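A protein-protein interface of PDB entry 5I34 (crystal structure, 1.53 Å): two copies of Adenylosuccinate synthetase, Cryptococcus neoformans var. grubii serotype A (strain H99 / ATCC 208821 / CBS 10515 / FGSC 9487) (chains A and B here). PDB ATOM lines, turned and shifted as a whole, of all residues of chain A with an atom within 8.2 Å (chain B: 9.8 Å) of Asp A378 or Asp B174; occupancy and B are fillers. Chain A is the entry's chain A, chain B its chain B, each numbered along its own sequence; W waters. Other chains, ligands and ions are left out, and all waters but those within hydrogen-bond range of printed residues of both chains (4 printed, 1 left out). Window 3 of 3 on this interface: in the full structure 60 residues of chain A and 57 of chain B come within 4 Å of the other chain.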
ATOM      1  N   TYR A 251      15.078  11.734  16.523  1.00  0.00           N
ATOM      2  CA  TYR A 251      14.421  12.753  15.702  1.00  0.00           C
ATOM      3  C   TYR A 251      13.450  13.585  16.544  1.00  0.00           C
ATOM      4  O   TYR A 251      12.657  13.016  17.291  1.00  0.00           O
ATOM      5  CB  TYR A 251      13.679  12.065  14.529  1.00  0.00           C
ATOM      6  CG  TYR A 251      13.017  13.009  13.565  1.00  0.00           C
ATOM      7  CD1 TYR A 251      11.779  13.577  13.855  1.00  0.00           C
ATOM      8  CD2 TYR A 251      13.608  13.315  12.344  1.00  0.00           C
ATOM      9  CE1 TYR A 251      11.170  14.439  12.968  1.00  0.00           C
ATOM     10  CE2 TYR A 251      13.002  14.185  11.458  1.00  0.00           C
ATOM     11  CZ  TYR A 251      11.783  14.740  11.771  1.00  0.00           C
ATOM     12  OH  TYR A 251      11.191  15.615  10.890  1.00  0.00           O
ATOM     13  N   PRO A 293      15.139  13.928  25.466  1.00  0.00           N
ATOM     14  CA  PRO A 293      15.477  12.987  26.538  1.00  0.00           C
ATOM     15  C   PRO A 293      16.867  12.358  26.412  1.00  0.00           C
ATOM     16  O   PRO A 293      17.463  12.269  25.329  1.00  0.00           O
ATOM     17  CB  PRO A 293      14.402  11.907  26.408  1.00  0.00           C
ATOM     18  CG  PRO A 293      13.293  12.556  25.681  1.00  0.00           C
ATOM     19  CD  PRO A 293      13.917  13.518  24.756  1.00  0.00           C
ATOM     20  N   ILE A 365       8.540   0.872  30.459  1.00  0.00           N
ATOM     21  CA  ILE A 365       7.499   1.892  30.455  1.00  0.00           C
ATOM     22  C   ILE A 365       6.258   1.258  31.042  1.00  0.00           C
ATOM     23  O   ILE A 365       5.815   0.196  30.592  1.00  0.00           O
ATOM     24  CB  ILE A 365       7.220   2.443  29.049  1.00  0.00           C
ATOM     25  CG1 ILE A 365       8.448   3.199  28.540  1.00  0.00           C
ATOM     26  CG2 ILE A 365       5.994   3.372  29.071  1.00  0.00           C
ATOM     27  CD1 ILE A 365       8.278   3.831  27.166  1.00  0.00           C
ATOM     28  N   PRO A 374      12.651   3.622  21.672  1.00  0.00           N
ATOM     29  CA  PRO A 374      11.382   4.214  21.219  1.00  0.00           C
ATOM     30  C   PRO A 374      11.549   5.417  20.282  1.00  0.00           C
ATOM     31  O   PRO A 374      12.358   6.323  20.550  1.00  0.00           O
ATOM     32  CB  PRO A 374      10.704   4.635  22.530  1.00  0.00           C
ATOM     33  CG  PRO A 374      11.795   4.839  23.486  1.00  0.00           C
ATOM     34  CD  PRO A 374      12.903   3.879  23.102  1.00  0.00           C
ATOM     35  N   ALA A 375      10.775   5.411  19.202  1.00  0.00           N
ATOM     36  CA  ALA A 375      10.733   6.507  18.237  1.00  0.00           C
ATOM     37  C   ALA A 375      10.054   7.745  18.828  1.00  0.00           C
ATOM     38  O   ALA A 375      10.355   8.864  18.447  1.00  0.00           O
ATOM     39  CB  ALA A 375       9.996   6.059  16.979  1.00  0.00           C
ATOM     40  N   ASP A 376       9.117   7.540  19.748  1.00  0.00           N
ATOM     41  CA  ASP A 376       8.360   8.632  20.358  1.00  0.00           C
ATOM     42  C   ASP A 376       9.117   9.166  21.572  1.00  0.00           C
ATOM     43  O   ASP A 376       9.402   8.420  22.514  1.00  0.00           O
ATOM     44  CB  ASP A 376       6.968   8.149  20.767  1.00  0.00           C
ATOM     45  CG  ASP A 376       6.076   9.286  21.278  1.00  0.00           C
ATOM     46  OD1 ASP A 376       6.475  10.002  22.208  1.00  0.00           O
ATOM     47  OD2 ASP A 376       4.955   9.459  20.766  1.00  0.00           O
ATOM     48  N   LEU A 377       9.463  10.443  21.542  1.00  0.00           N
ATOM     49  CA  LEU A 377      10.297  11.011  22.595  1.00  0.00           C
ATOM     50  C   LEU A 377       9.525  11.232  23.874  1.00  0.00           C
ATOM     51  O   LEU A 377      10.123  11.343  24.943  1.00  0.00           O
ATOM     52  CB  LEU A 377      10.935  12.325  22.141  1.00  0.00           C
ATOM     53  CG  LEU A 377      11.888  12.247  20.943  1.00  0.00           C
ATOM     54  CD1 LEU A 377      12.553  13.594  20.646  1.00  0.00           C
ATOM     55  CD2 LEU A 377      12.982  11.212  21.196  1.00  0.00           C
ATOM     56  N   ASP A 378       8.201  11.272  23.795  1.00  0.00           N
ATOM     57  CA  ASP A 378       7.437  11.364  25.023  1.00  0.00           C
ATOM     58  C   ASP A 378       7.447  10.000  25.721  1.00  0.00           C
ATOM     59  O   ASP A 378       7.486   9.932  26.953  1.00  0.00           O
ATOM     60  CB  ASP A 378       6.028  11.855  24.748  1.00  0.00           C
ATOM     61  CG  ASP A 378       6.011  13.291  24.269  1.00  0.00           C
ATOM     62  OD1 ASP A 378       6.718  14.132  24.870  1.00  0.00           O
ATOM     63  OD2 ASP A 378       5.297  13.583  23.302  1.00  0.00           O
ATOM     64  N   ARG A 379       7.466   8.914  24.953  1.00  0.00           N
ATOM     65  CA  ARG A 379       7.651   7.603  25.555  1.00  0.00           C
ATOM     66  C   ARG A 379       9.064   7.475  26.112  1.00  0.00           C
ATOM     67  O   ARG A 379       9.234   6.953  27.222  1.00  0.00           O
ATOM     68  CB  ARG A 379       7.371   6.482  24.557  1.00  0.00           C
ATOM     69  CG  ARG A 379       5.921   6.389  24.144  1.00  0.00           C
ATOM     70  CD  ARG A 379       5.650   5.117  23.363  1.00  0.00           C
ATOM     71  NE  ARG A 379       5.838   3.917  24.180  1.00  0.00           N
ATOM     72  CZ  ARG A 379       6.605   2.876  23.855  1.00  0.00           C
ATOM     73  NH1 ARG A 379       7.291   2.859  22.713  1.00  0.00           N
ATOM     74  NH2 ARG A 379       6.680   1.838  24.681  1.00  0.00           N
ATOM     75  N   LEU A 380      10.058   7.966  25.363  1.00  0.00           N
ATOM     76  CA  LEU A 380      11.451   7.938  25.818  1.00  0.00           C
ATOM     77  C   LEU A 380      11.590   8.682  27.146  1.00  0.00           C
ATOM     78  O   LEU A 380      12.322   8.242  28.037  1.00  0.00           O
ATOM     79  CB  LEU A 380      12.383   8.547  24.770  1.00  0.00           C
ATOM     80  CG  LEU A 380      13.887   8.423  25.090  1.00  0.00           C
ATOM     81  CD1 LEU A 380      14.347   6.957  25.190  1.00  0.00           C
ATOM     82  CD2 LEU A 380      14.717   9.173  24.058  1.00  0.00           C
ATOM     83  N   ALA A 381      10.872   9.792  27.279  1.00  0.00           N
ATOM     84  CA  ALA A 381      10.921  10.602  28.496  1.00  0.00           C
ATOM     85  C   ALA A 381      10.389   9.841  29.706  1.00  0.00           C
ATOM     86  O   ALA A 381      10.770  10.135  30.840  1.00  0.00           O
ATOM     87  CB  ALA A 381      10.127  11.902  28.306  1.00  0.00           C
ATOM     88  N   LYS A 382       9.513   8.867  29.463  1.00  0.00           N
ATOM     89  CA  LYS A 382       8.875   8.093  30.542  1.00  0.00           C
ATOM     90  C   LYS A 382       9.666   6.877  31.014  1.00  0.00           C
ATOM     91  O   LYS A 382       9.275   6.222  31.970  1.00  0.00           O
ATOM     92  CB  LYS A 382       7.506   7.600  30.087  1.00  0.00           C
ATOM     93  CG  LYS A 382       6.472   8.679  29.891  1.00  0.00           C
ATOM     94  CD  LYS A 382       5.219   8.126  29.216  1.00  0.00           C
ATOM     95  CE  LYS A 382       4.484   7.130  30.095  1.00  0.00           C
ATOM     96  NZ  LYS A 382       3.236   6.639  29.442  1.00  0.00           N
ATOM     97  N   VAL A 383      10.754   6.556  30.326  1.00  0.00           N
ATOM     98  CA  VAL A 383      11.455   5.299  30.550  1.00  0.00           C
ATOM     99  C   VAL A 383      11.966   5.205  31.976  1.00  0.00           C
ATOM    100  O   VAL A 383      12.502   6.165  32.518  1.00  0.00           O
ATOM    101  CB  VAL A 383      12.626   5.136  29.558  1.00  0.00           C
ATOM    102  CG1 VAL A 383      13.628   4.098  30.040  1.00  0.00           C
ATOM    103  CG2 VAL A 383      12.098   4.745  28.177  1.00  0.00           C
ATOM    104  N   LEU B 126       5.222  11.506   7.222  1.00  0.00           N
ATOM    105  CA  LEU B 126       3.868  11.756   6.768  1.00  0.00           C
ATOM    106  C   LEU B 126       3.828  12.806   5.659  1.00  0.00           C
ATOM    107  O   LEU B 126       4.317  13.925   5.823  1.00  0.00           O
ATOM    108  CB  LEU B 126       3.002  12.235   7.936  1.00  0.00           C
ATOM    109  CG  LEU B 126       2.885  11.299   9.134  1.00  0.00           C
ATOM    110  CD1 LEU B 126       2.029  11.954  10.210  1.00  0.00           C
ATOM    111  CD2 LEU B 126       2.298   9.955   8.736  1.00  0.00           C
ATOM    112  N   GLY B 166       9.502  17.922   9.554  1.00  0.00           N
ATOM    113  CA  GLY B 166       8.497  16.961   9.133  1.00  0.00           C
ATOM    114  C   GLY B 166       7.917  16.148  10.269  1.00  0.00           C
ATOM    115  O   GLY B 166       8.557  15.991  11.313  1.00  0.00           O
ATOM    116  N   LEU B 167       6.706  15.625  10.058  1.00  0.00           N
ATOM    117  CA  LEU B 167       6.019  14.816  11.054  1.00  0.00           C
ATOM    118  C   LEU B 167       6.063  13.356  10.629  1.00  0.00           C
ATOM    119  O   LEU B 167       6.056  13.045   9.429  1.00  0.00           O
ATOM    120  CB  LEU B 167       4.578  15.299  11.249  1.00  0.00           C
ATOM    121  CG  LEU B 167       4.509  16.756  11.726  1.00  0.00           C
ATOM    122  CD1 LEU B 167       3.075  17.210  11.819  1.00  0.00           C
ATOM    123  CD2 LEU B 167       5.201  16.955  13.084  1.00  0.00           C
ATOM    124  N   ARG B 168       6.106  12.473  11.619  1.00  0.00           N
ATOM    125  CA  ARG B 168       6.291  11.050  11.405  1.00  0.00           C
ATOM    126  C   ARG B 168       5.077  10.333  11.987  1.00  0.00           C
ATOM    127  O   ARG B 168       4.246  10.927  12.672  1.00  0.00           O
ATOM    128  CB  ARG B 168       7.594  10.560  12.047  1.00  0.00           C
ATOM    129  CG  ARG B 168       8.824  11.441  11.713  1.00  0.00           C
ATOM    130  CD  ARG B 168      10.157  10.753  11.964  1.00  0.00           C
ATOM    131  NE  ARG B 168      10.266  10.268  13.334  1.00  0.00           N
ATOM    132  CZ  ARG B 168      11.292   9.570  13.802  1.00  0.00           C
ATOM    133  NH1 ARG B 168      12.317   9.306  13.008  1.00  0.00           N
ATOM    134  NH2 ARG B 168      11.316   9.147  15.065  1.00  0.00           N
ATOM    135  N   VAL B 169       4.955   9.053  11.679  1.00  0.00           N
ATOM    136  CA  VAL B 169       3.812   8.262  12.103  1.00  0.00           C
ATOM    137  C   VAL B 169       3.551   8.405  13.618  1.00  0.00           C
ATOM    138  O   VAL B 169       2.399   8.565  14.036  1.00  0.00           O
ATOM    139  CB  VAL B 169       4.026   6.791  11.701  1.00  0.00           C
ATOM    140  CG1 VAL B 169       3.093   5.886  12.422  1.00  0.00           C
ATOM    141  CG2 VAL B 169       3.832   6.609  10.188  1.00  0.00           C
ATOM    142  N   HIS B 170       4.597   8.362  14.458  1.00  0.00           N
ATOM    143  CA  HIS B 170       4.372   8.455  15.902  1.00  0.00           C
ATOM    144  C   HIS B 170       3.744   9.796  16.313  1.00  0.00           C
ATOM    145  O   HIS B 170       3.032   9.880  17.337  1.00  0.00           O
ATOM    146  CB  HIS B 170       5.673   8.212  16.690  1.00  0.00           C
ATOM    147  CG  HIS B 170       6.755   9.200  16.414  1.00  0.00           C
ATOM    148  ND1 HIS B 170       6.824  10.436  17.031  1.00  0.00           N
ATOM    149  CD2 HIS B 170       7.822   9.129  15.588  1.00  0.00           C
ATOM    150  CE1 HIS B 170       7.890  11.080  16.590  1.00  0.00           C
ATOM    151  NE2 HIS B 170       8.508  10.313  15.706  1.00  0.00           N
ATOM    152  N   HIS B 171       3.969  10.843  15.522  1.00  0.00           N
ATOM    153  CA  HIS B 171       3.378  12.140  15.843  1.00  0.00           C
ATOM    154  C   HIS B 171       1.858  12.122  15.773  1.00  0.00           C
ATOM    155  O   HIS B 171       1.216  12.995  16.355  1.00  0.00           O
ATOM    156  CB  HIS B 171       3.890  13.230  14.907  1.00  0.00           C
ATOM    157  CG  HIS B 171       5.277  13.696  15.221  1.00  0.00           C
ATOM    158  ND1 HIS B 171       6.346  13.514  14.371  1.00  0.00           N
ATOM    159  CD2 HIS B 171       5.760  14.344  16.307  1.00  0.00           C
ATOM    160  CE1 HIS B 171       7.427  14.048  14.918  1.00  0.00           C
ATOM    161  NE2 HIS B 171       7.094  14.558  16.093  1.00  0.00           N
ATOM    162  N   LEU B 172       1.268  11.141  15.091  1.00  0.00           N
ATOM    163  CA  LEU B 172      -0.189  11.062  15.021  1.00  0.00           C
ATOM    164  C   LEU B 172      -0.842  10.854  16.386  1.00  0.00           C
ATOM    165  O   LEU B 172      -2.051  11.046  16.518  1.00  0.00           O
ATOM    166  CB  LEU B 172      -0.628   9.944  14.077  1.00  0.00           C
ATOM    167  CG  LEU B 172      -0.312  10.167  12.599  1.00  0.00           C
ATOM    168  CD1 LEU B 172      -0.496   8.861  11.837  1.00  0.00           C
ATOM    169  CD2 LEU B 172      -1.212  11.264  12.042  1.00  0.00           C
ATOM    170  N   PHE B 173      -0.059  10.451  17.390  1.00  0.00           N
ATOM    171  CA  PHE B 173      -0.572  10.212  18.739  1.00  0.00           C
ATOM    172  C   PHE B 173      -0.015  11.214  19.740  1.00  0.00           C
ATOM    173  O   PHE B 173      -0.206  11.078  20.944  1.00  0.00           O
ATOM    174  CB  PHE B 173      -0.248   8.779  19.135  1.00  0.00           C
ATOM    175  CG  PHE B 173      -0.698   7.797  18.111  1.00  0.00           C
ATOM    176  CD1 PHE B 173      -2.025   7.406  18.055  1.00  0.00           C
ATOM    177  CD2 PHE B 173       0.170   7.336  17.146  1.00  0.00           C
ATOM    178  CE1 PHE B 173      -2.458   6.535  17.078  1.00  0.00           C
ATOM    179  CE2 PHE B 173      -0.269   6.469  16.162  1.00  0.00           C
ATOM    180  CZ  PHE B 173      -1.581   6.065  16.135  1.00  0.00           C
ATOM    181  N   ASP B 174       0.629  12.243  19.208  1.00  0.00           N
ATOM    182  CA  ASP B 174       1.294  13.290  19.971  1.00  0.00           C
ATOM    183  C   ASP B 174       0.353  14.484  20.107  1.00  0.00           C
ATOM    184  O   ASP B 174      -0.155  14.968  19.113  1.00  0.00           O
ATOM    185  CB  ASP B 174       2.584  13.649  19.216  1.00  0.00           C
ATOM    186  CG  ASP B 174       3.468  14.656  19.913  1.00  0.00           C
ATOM    187  OD1 ASP B 174       2.990  15.528  20.684  1.00  0.00           O
ATOM    188  OD2 ASP B 174       4.686  14.586  19.619  1.00  0.00           O
ATOM    189  N   PRO B 175       0.092  14.950  21.340  1.00  0.00           N
ATOM    190  CA  PRO B 175      -0.874  16.048  21.482  1.00  0.00           C
ATOM    191  C   PRO B 175      -0.430  17.346  20.803  1.00  0.00           C
ATOM    192  O   PRO B 175      -1.260  18.227  20.596  1.00  0.00           O
ATOM    193  CB  PRO B 175      -0.964  16.239  22.989  1.00  0.00           C
ATOM    194  CG  PRO B 175       0.321  15.725  23.512  1.00  0.00           C
ATOM    195  CD  PRO B 175       0.659  14.549  22.642  1.00  0.00           C
ATOM    196  N   THR B 176       0.854  17.454  20.457  1.00  0.00           N
ATOM    197  CA  THR B 176       1.358  18.645  19.778  1.00  0.00           C
ATOM    198  C   THR B 176       1.229  18.570  18.259  1.00  0.00           C
ATOM    199  O   THR B 176       1.654  19.499  17.572  1.00  0.00           O
ATOM    200  CB  THR B 176       2.855  18.935  20.108  1.00  0.00           C
ATOM    201  OG1 THR B 176       3.710  17.939  19.522  1.00  0.00           O
ATOM    202  CG2 THR B 176       3.077  19.007  21.602  1.00  0.00           C
ATOM    203  N   PHE B 177       0.653  17.490  17.732  1.00  0.00           N
ATOM    204  CA  PHE B 177       0.522  17.332  16.277  1.00  0.00           C
ATOM    205  C   PHE B 177      -0.199  18.522  15.652  1.00  0.00           C
ATOM    206  O   PHE B 177       0.292  19.104  14.689  1.00  0.00           O
ATOM    207  CB  PHE B 177      -0.197  16.014  15.933  1.00  0.00           C
ATOM    208  CG  PHE B 177      -0.477  15.834  14.467  1.00  0.00           C
ATOM    209  CD1 PHE B 177       0.422  15.164  13.653  1.00  0.00           C
ATOM    210  CD2 PHE B 177      -1.645  16.317  13.905  1.00  0.00           C
ATOM    211  CE1 PHE B 177       0.153  14.994  12.288  1.00  0.00           C
ATOM    212  CE2 PHE B 177      -1.918  16.145  12.557  1.00  0.00           C
ATOM    213  CZ  PHE B 177      -1.010  15.474  11.750  1.00  0.00           C
ATOM    214  N   PRO B 178      -1.345  18.927  16.210  1.00  0.00           N
ATOM    215  CA  PRO B 178      -2.010  20.074  15.577  1.00  0.00           C
ATOM    216  C   PRO B 178      -1.171  21.351  15.540  1.00  0.00           C
ATOM    217  O   PRO B 178      -1.120  22.004  14.502  1.00  0.00           O
ATOM    218  CB  PRO B 178      -3.239  20.271  16.451  1.00  0.00           C
ATOM    219  CG  PRO B 178      -3.525  18.907  16.991  1.00  0.00           C
ATOM    220  CD  PRO B 178      -2.180  18.350  17.285  1.00  0.00           C
ATOM    221  N   ALA B 179      -0.529  21.699  16.647  1.00  0.00           N
ATOM    222  CA  ALA B 179       0.292  22.895  16.684  1.00  0.00           C
ATOM    223  C   ALA B 179       1.432  22.800  15.686  1.00  0.00           C
ATOM    224  O   ALA B 179       1.742  23.769  14.991  1.00  0.00           O
ATOM    225  CB  ALA B 179       0.840  23.132  18.091  1.00  0.00           C
ATOM    226  N   LYS B 180       2.057  21.633  15.601  1.00  0.00           N
ATOM    227  CA  LYS B 180       3.183  21.462  14.689  1.00  0.00           C
ATOM    228  C   LYS B 180       2.701  21.528  13.237  1.00  0.00           C
ATOM    229  O   LYS B 180       3.368  22.112  12.380  1.00  0.00           O
ATOM    230  CB  LYS B 180       3.909  20.152  14.964  1.00  0.00           C
ATOM    231  CG  LYS B 180       4.820  20.183  16.187  1.00  0.00           C
ATOM    232  CD  LYS B 180       5.442  18.802  16.459  1.00  0.00           C
ATOM    233  CE  LYS B 180       6.566  18.888  17.500  1.00  0.00           C
ATOM    234  NZ  LYS B 180       6.117  19.247  18.861  1.00  0.00           N
ATOM    235  N   PHE B 181       1.548  20.934  12.965  1.00  0.00           N
ATOM    236  CA  PHE B 181       0.951  20.992  11.626  1.00  0.00           C
ATOM    237  C   PHE B 181       0.650  22.446  11.185  1.00  0.00           C
ATOM    238  O   PHE B 181       0.964  22.854  10.061  1.00  0.00           O
ATOM    239  CB  PHE B 181      -0.325  20.140  11.632  1.00  0.00           C
ATOM    240  CG  PHE B 181      -0.954  19.941  10.285  1.00  0.00           C
ATOM    241  CD1 PHE B 181      -1.679  20.955   9.688  1.00  0.00           C
ATOM    242  CD2 PHE B 181      -0.885  18.708   9.649  1.00  0.00           C
ATOM    243  CE1 PHE B 181      -2.292  20.761   8.454  1.00  0.00           C
ATOM    244  CE2 PHE B 181      -1.504  18.505   8.421  1.00  0.00           C
ATOM    245  CZ  PHE B 181      -2.206  19.541   7.822  1.00  0.00           C
ATOM    246  N   ARG B 182       0.063  23.223  12.084  1.00  0.00           N
ATOM    247  CA  ARG B 182      -0.235  24.628  11.808  1.00  0.00           C
ATOM    248  C   ARG B 182       1.023  25.412  11.472  1.00  0.00           C
ATOM    249  O   ARG B 182       1.013  26.223  10.548  1.00  0.00           O
ATOM    250  CB  ARG B 182      -0.942  25.259  13.005  1.00  0.00           C
ATOM    251  CG  ARG B 182      -2.341  24.741  13.173  1.00  0.00           C
ATOM    252  CD  ARG B 182      -3.001  25.243  14.434  1.00  0.00           C
ATOM    253  NE  ARG B 182      -4.254  24.527  14.685  1.00  0.00           N
ATOM    254  CZ  ARG B 182      -4.516  23.790  15.763  1.00  0.00           C
ATOM    255  NH1 ARG B 182      -3.651  23.699  16.761  1.00  0.00           N
ATOM    256  NH2 ARG B 182      -5.680  23.164  15.856  1.00  0.00           N
ATOM    257  N   ILE B 203      -6.336  18.456   9.799  1.00  0.00           N
ATOM    258  CA  ILE B 203      -5.830  17.936  11.054  1.00  0.00           C
ATOM    259  C   ILE B 203      -6.840  16.936  11.578  1.00  0.00           C
ATOM    260  O   ILE B 203      -6.482  15.811  11.917  1.00  0.00           O
ATOM    261  CB  ILE B 203      -5.574  19.057  12.085  1.00  0.00           C
ATOM    262  CG1 ILE B 203      -4.362  19.886  11.653  1.00  0.00           C
ATOM    263  CG2 ILE B 203      -5.304  18.476  13.465  1.00  0.00           C
ATOM    264  CD1 ILE B 203      -4.179  21.169  12.450  1.00  0.00           C
ATOM    265  N   LEU B 207      -6.065  12.775  12.318  1.00  0.00           N
ATOM    266  CA  LEU B 207      -6.147  12.179  13.635  1.00  0.00           C
ATOM    267  C   LEU B 207      -7.201  11.088  13.612  1.00  0.00           C
ATOM    268  O   LEU B 207      -7.110  10.132  14.369  1.00  0.00           O
ATOM    269  CB  LEU B 207      -6.463  13.233  14.705  1.00  0.00           C
ATOM    270  CG  LEU B 207      -5.234  13.990  15.232  1.00  0.00           C
ATOM    271  CD1 LEU B 207      -4.486  14.594  14.102  1.00  0.00           C
ATOM    272  CD2 LEU B 207      -5.600  15.085  16.235  1.00  0.00           C
ATOM    273  N   ALA B 210      -5.644   8.096  12.413  1.00  0.00           N
ATOM    274  CA  ALA B 210      -4.655   7.599  13.360  1.00  0.00           C
ATOM    275  C   ALA B 210      -5.201   6.402  14.128  1.00  0.00           C
ATOM    276  O   ALA B 210      -4.468   5.454  14.427  1.00  0.00           O
ATOM    277  CB  ALA B 210      -4.234   8.685  14.321  1.00  0.00           C
ATOM    278  N   GLU B 211      -6.496   6.436  14.431  1.00  0.00           N
ATOM    279  CA  GLU B 211      -7.106   5.363  15.194  1.00  0.00           C
ATOM    280  C   GLU B 211      -7.116   4.084  14.375  1.00  0.00           C
ATOM    281  O   GLU B 211      -6.918   2.997  14.916  1.00  0.00           O
ATOM    282  CB  GLU B 211      -8.523   5.747  15.625  1.00  0.00           C
ATOM    283  CG  GLU B 211      -8.577   6.979  16.517  1.00  0.00           C
ATOM    284  CD  GLU B 211      -7.893   6.774  17.863  1.00  0.00           C
ATOM    285  OE1 GLU B 211      -7.583   5.614  18.217  1.00  0.00           O
ATOM    286  OE2 GLU B 211      -7.664   7.783  18.568  1.00  0.00           O
ATOM    287  N   ARG B 214      -3.342   2.690  14.134  1.00  0.00           N
ATOM    288  CA  ARG B 214      -2.713   2.247  15.375  1.00  0.00           C
ATOM    289  C   ARG B 214      -2.300   0.769  15.378  1.00  0.00           C
ATOM    290  O   ARG B 214      -1.159   0.452  15.712  1.00  0.00           O
ATOM    291  CB  ARG B 214      -3.651   2.533  16.554  1.00  0.00           C
ATOM    292  CG  ARG B 214      -2.984   2.453  17.924  1.00  0.00           C
ATOM    293  CD  ARG B 214      -3.999   2.527  19.056  1.00  0.00           C
ATOM    294  NE  ARG B 214      -4.640   3.839  19.154  1.00  0.00           N
ATOM    295  CZ  ARG B 214      -4.106   4.892  19.772  1.00  0.00           C
ATOM    296  NH1 ARG B 214      -2.911   4.796  20.338  1.00  0.00           N
ATOM    297  NH2 ARG B 214      -4.766   6.048  19.816  1.00  0.00           N
HETATM  298  O   HOH W   1       5.752  11.985  19.192  1.00  0.00           O
HETATM  299  O   HOH W   2      12.661  10.138  17.669  1.00  0.00           O
HETATM  300  O   HOH W   3       4.592  15.881  22.898  1.00  0.00           O
HETATM  301  O   HOH W   4       9.970  13.539  17.735  1.00  0.00           O
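The backbone carbonyl oxygen of Gly B166 lies within hydrogen-bond range of the side-chain hydroxyl of Tyr A251, at 2.7 Å.
The backbone NH (N) of Asp A378 sits at hydrogen-bond distance from the side-chain carboxylate (OD1) of Asp A376, at 2.7 Å.
The backbone NH (N) of Arg A379 sits at hydrogen-bond distance from the side-chain carboxylate (OD1) of Asp A376, at 3.1 Å.
NE2 of His B170 is in hydrogen-bond range of NE of Arg B168, 3.0 Å away.
The backbone NH (N) of Arg B168 lies within hydrogen-bond range of a ring nitrogen (ND1) of His B171, at 3.0 Å.
The side-chain hydroxyl (OG1) of Thr B176 lies within hydrogen-bond range of the side-chain carboxylate (OD1) of Asp B174 (2.8 Å).
Among the printed residues, merely in contact across the chains: Tyr A251 with Arg B168 (3.4 Å), Ala A375 with Arg B168 (3.5 Å), Ala A375 with His B170 (3.6 Å), Asp A378 with Asp B174 (3.9 Å) and Asp A376 with His B170 (3.95 Å).
Printed residues of chain B within 4 Å of Tyr A251: Gly B166 (2.7 Å) and Arg B168 (3.4 Å).
Of the printed residues of chain B, Ala A375 touches Arg B168 (3.5 Å) and His B170 (3.6 Å).
Asp A376 touches one residue of chain B.
Asp A378 touches one residue of chain B.
Ala A381 touches none of the printed residues of chain B.
Of the printed residues of chain A, Gly B166 touches Tyr A251.
Of the printed residues of chain A, His B170 touches Ala A375 (3.6 Å) and Asp A376 (3.95 Å).
Asp B174 touches just one residue of chain A: Asp A378 (3.9 Å).
Pro B175 touches none of the printed residues of chain A.
The nearest residue of chain A that does not touch Asp B174 is Asp A376 (5.1 Å).
The nearest printed residue of chain B that does not touch Tyr A251 is His B171 (4.2 Å).
Of the 13 printed residues of chain A, 4 touch a printed residue of chain B.
Hydrophobic or aromatic side chains of chain B that line the printed part of chain A: His B170.
Among the printed residues, no Asp or Glu carboxylate lies within 4 Å of a Lys or Arg side-chain nitrogen of the other chain.
No position is printed for both chains.
Water W3 bridges the side-chain carboxylate of Asp A378 and the side-chain carboxylate of Asp B174.
Water W2 lies within hydrogen-bond range of O of Ala A375 (2.7 Å), O of Tyr A251 (2.9 Å) and NH2 of Arg B168 (3.1 Å).
Water W4 bridges O of Tyr A251 (2.8 Å) and NE2 of His B171 (3.5 Å).
Water W1 lies within hydrogen-bond range of OD2 of Asp B174, ND1 of His B170 and OD2 of Asp A376.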
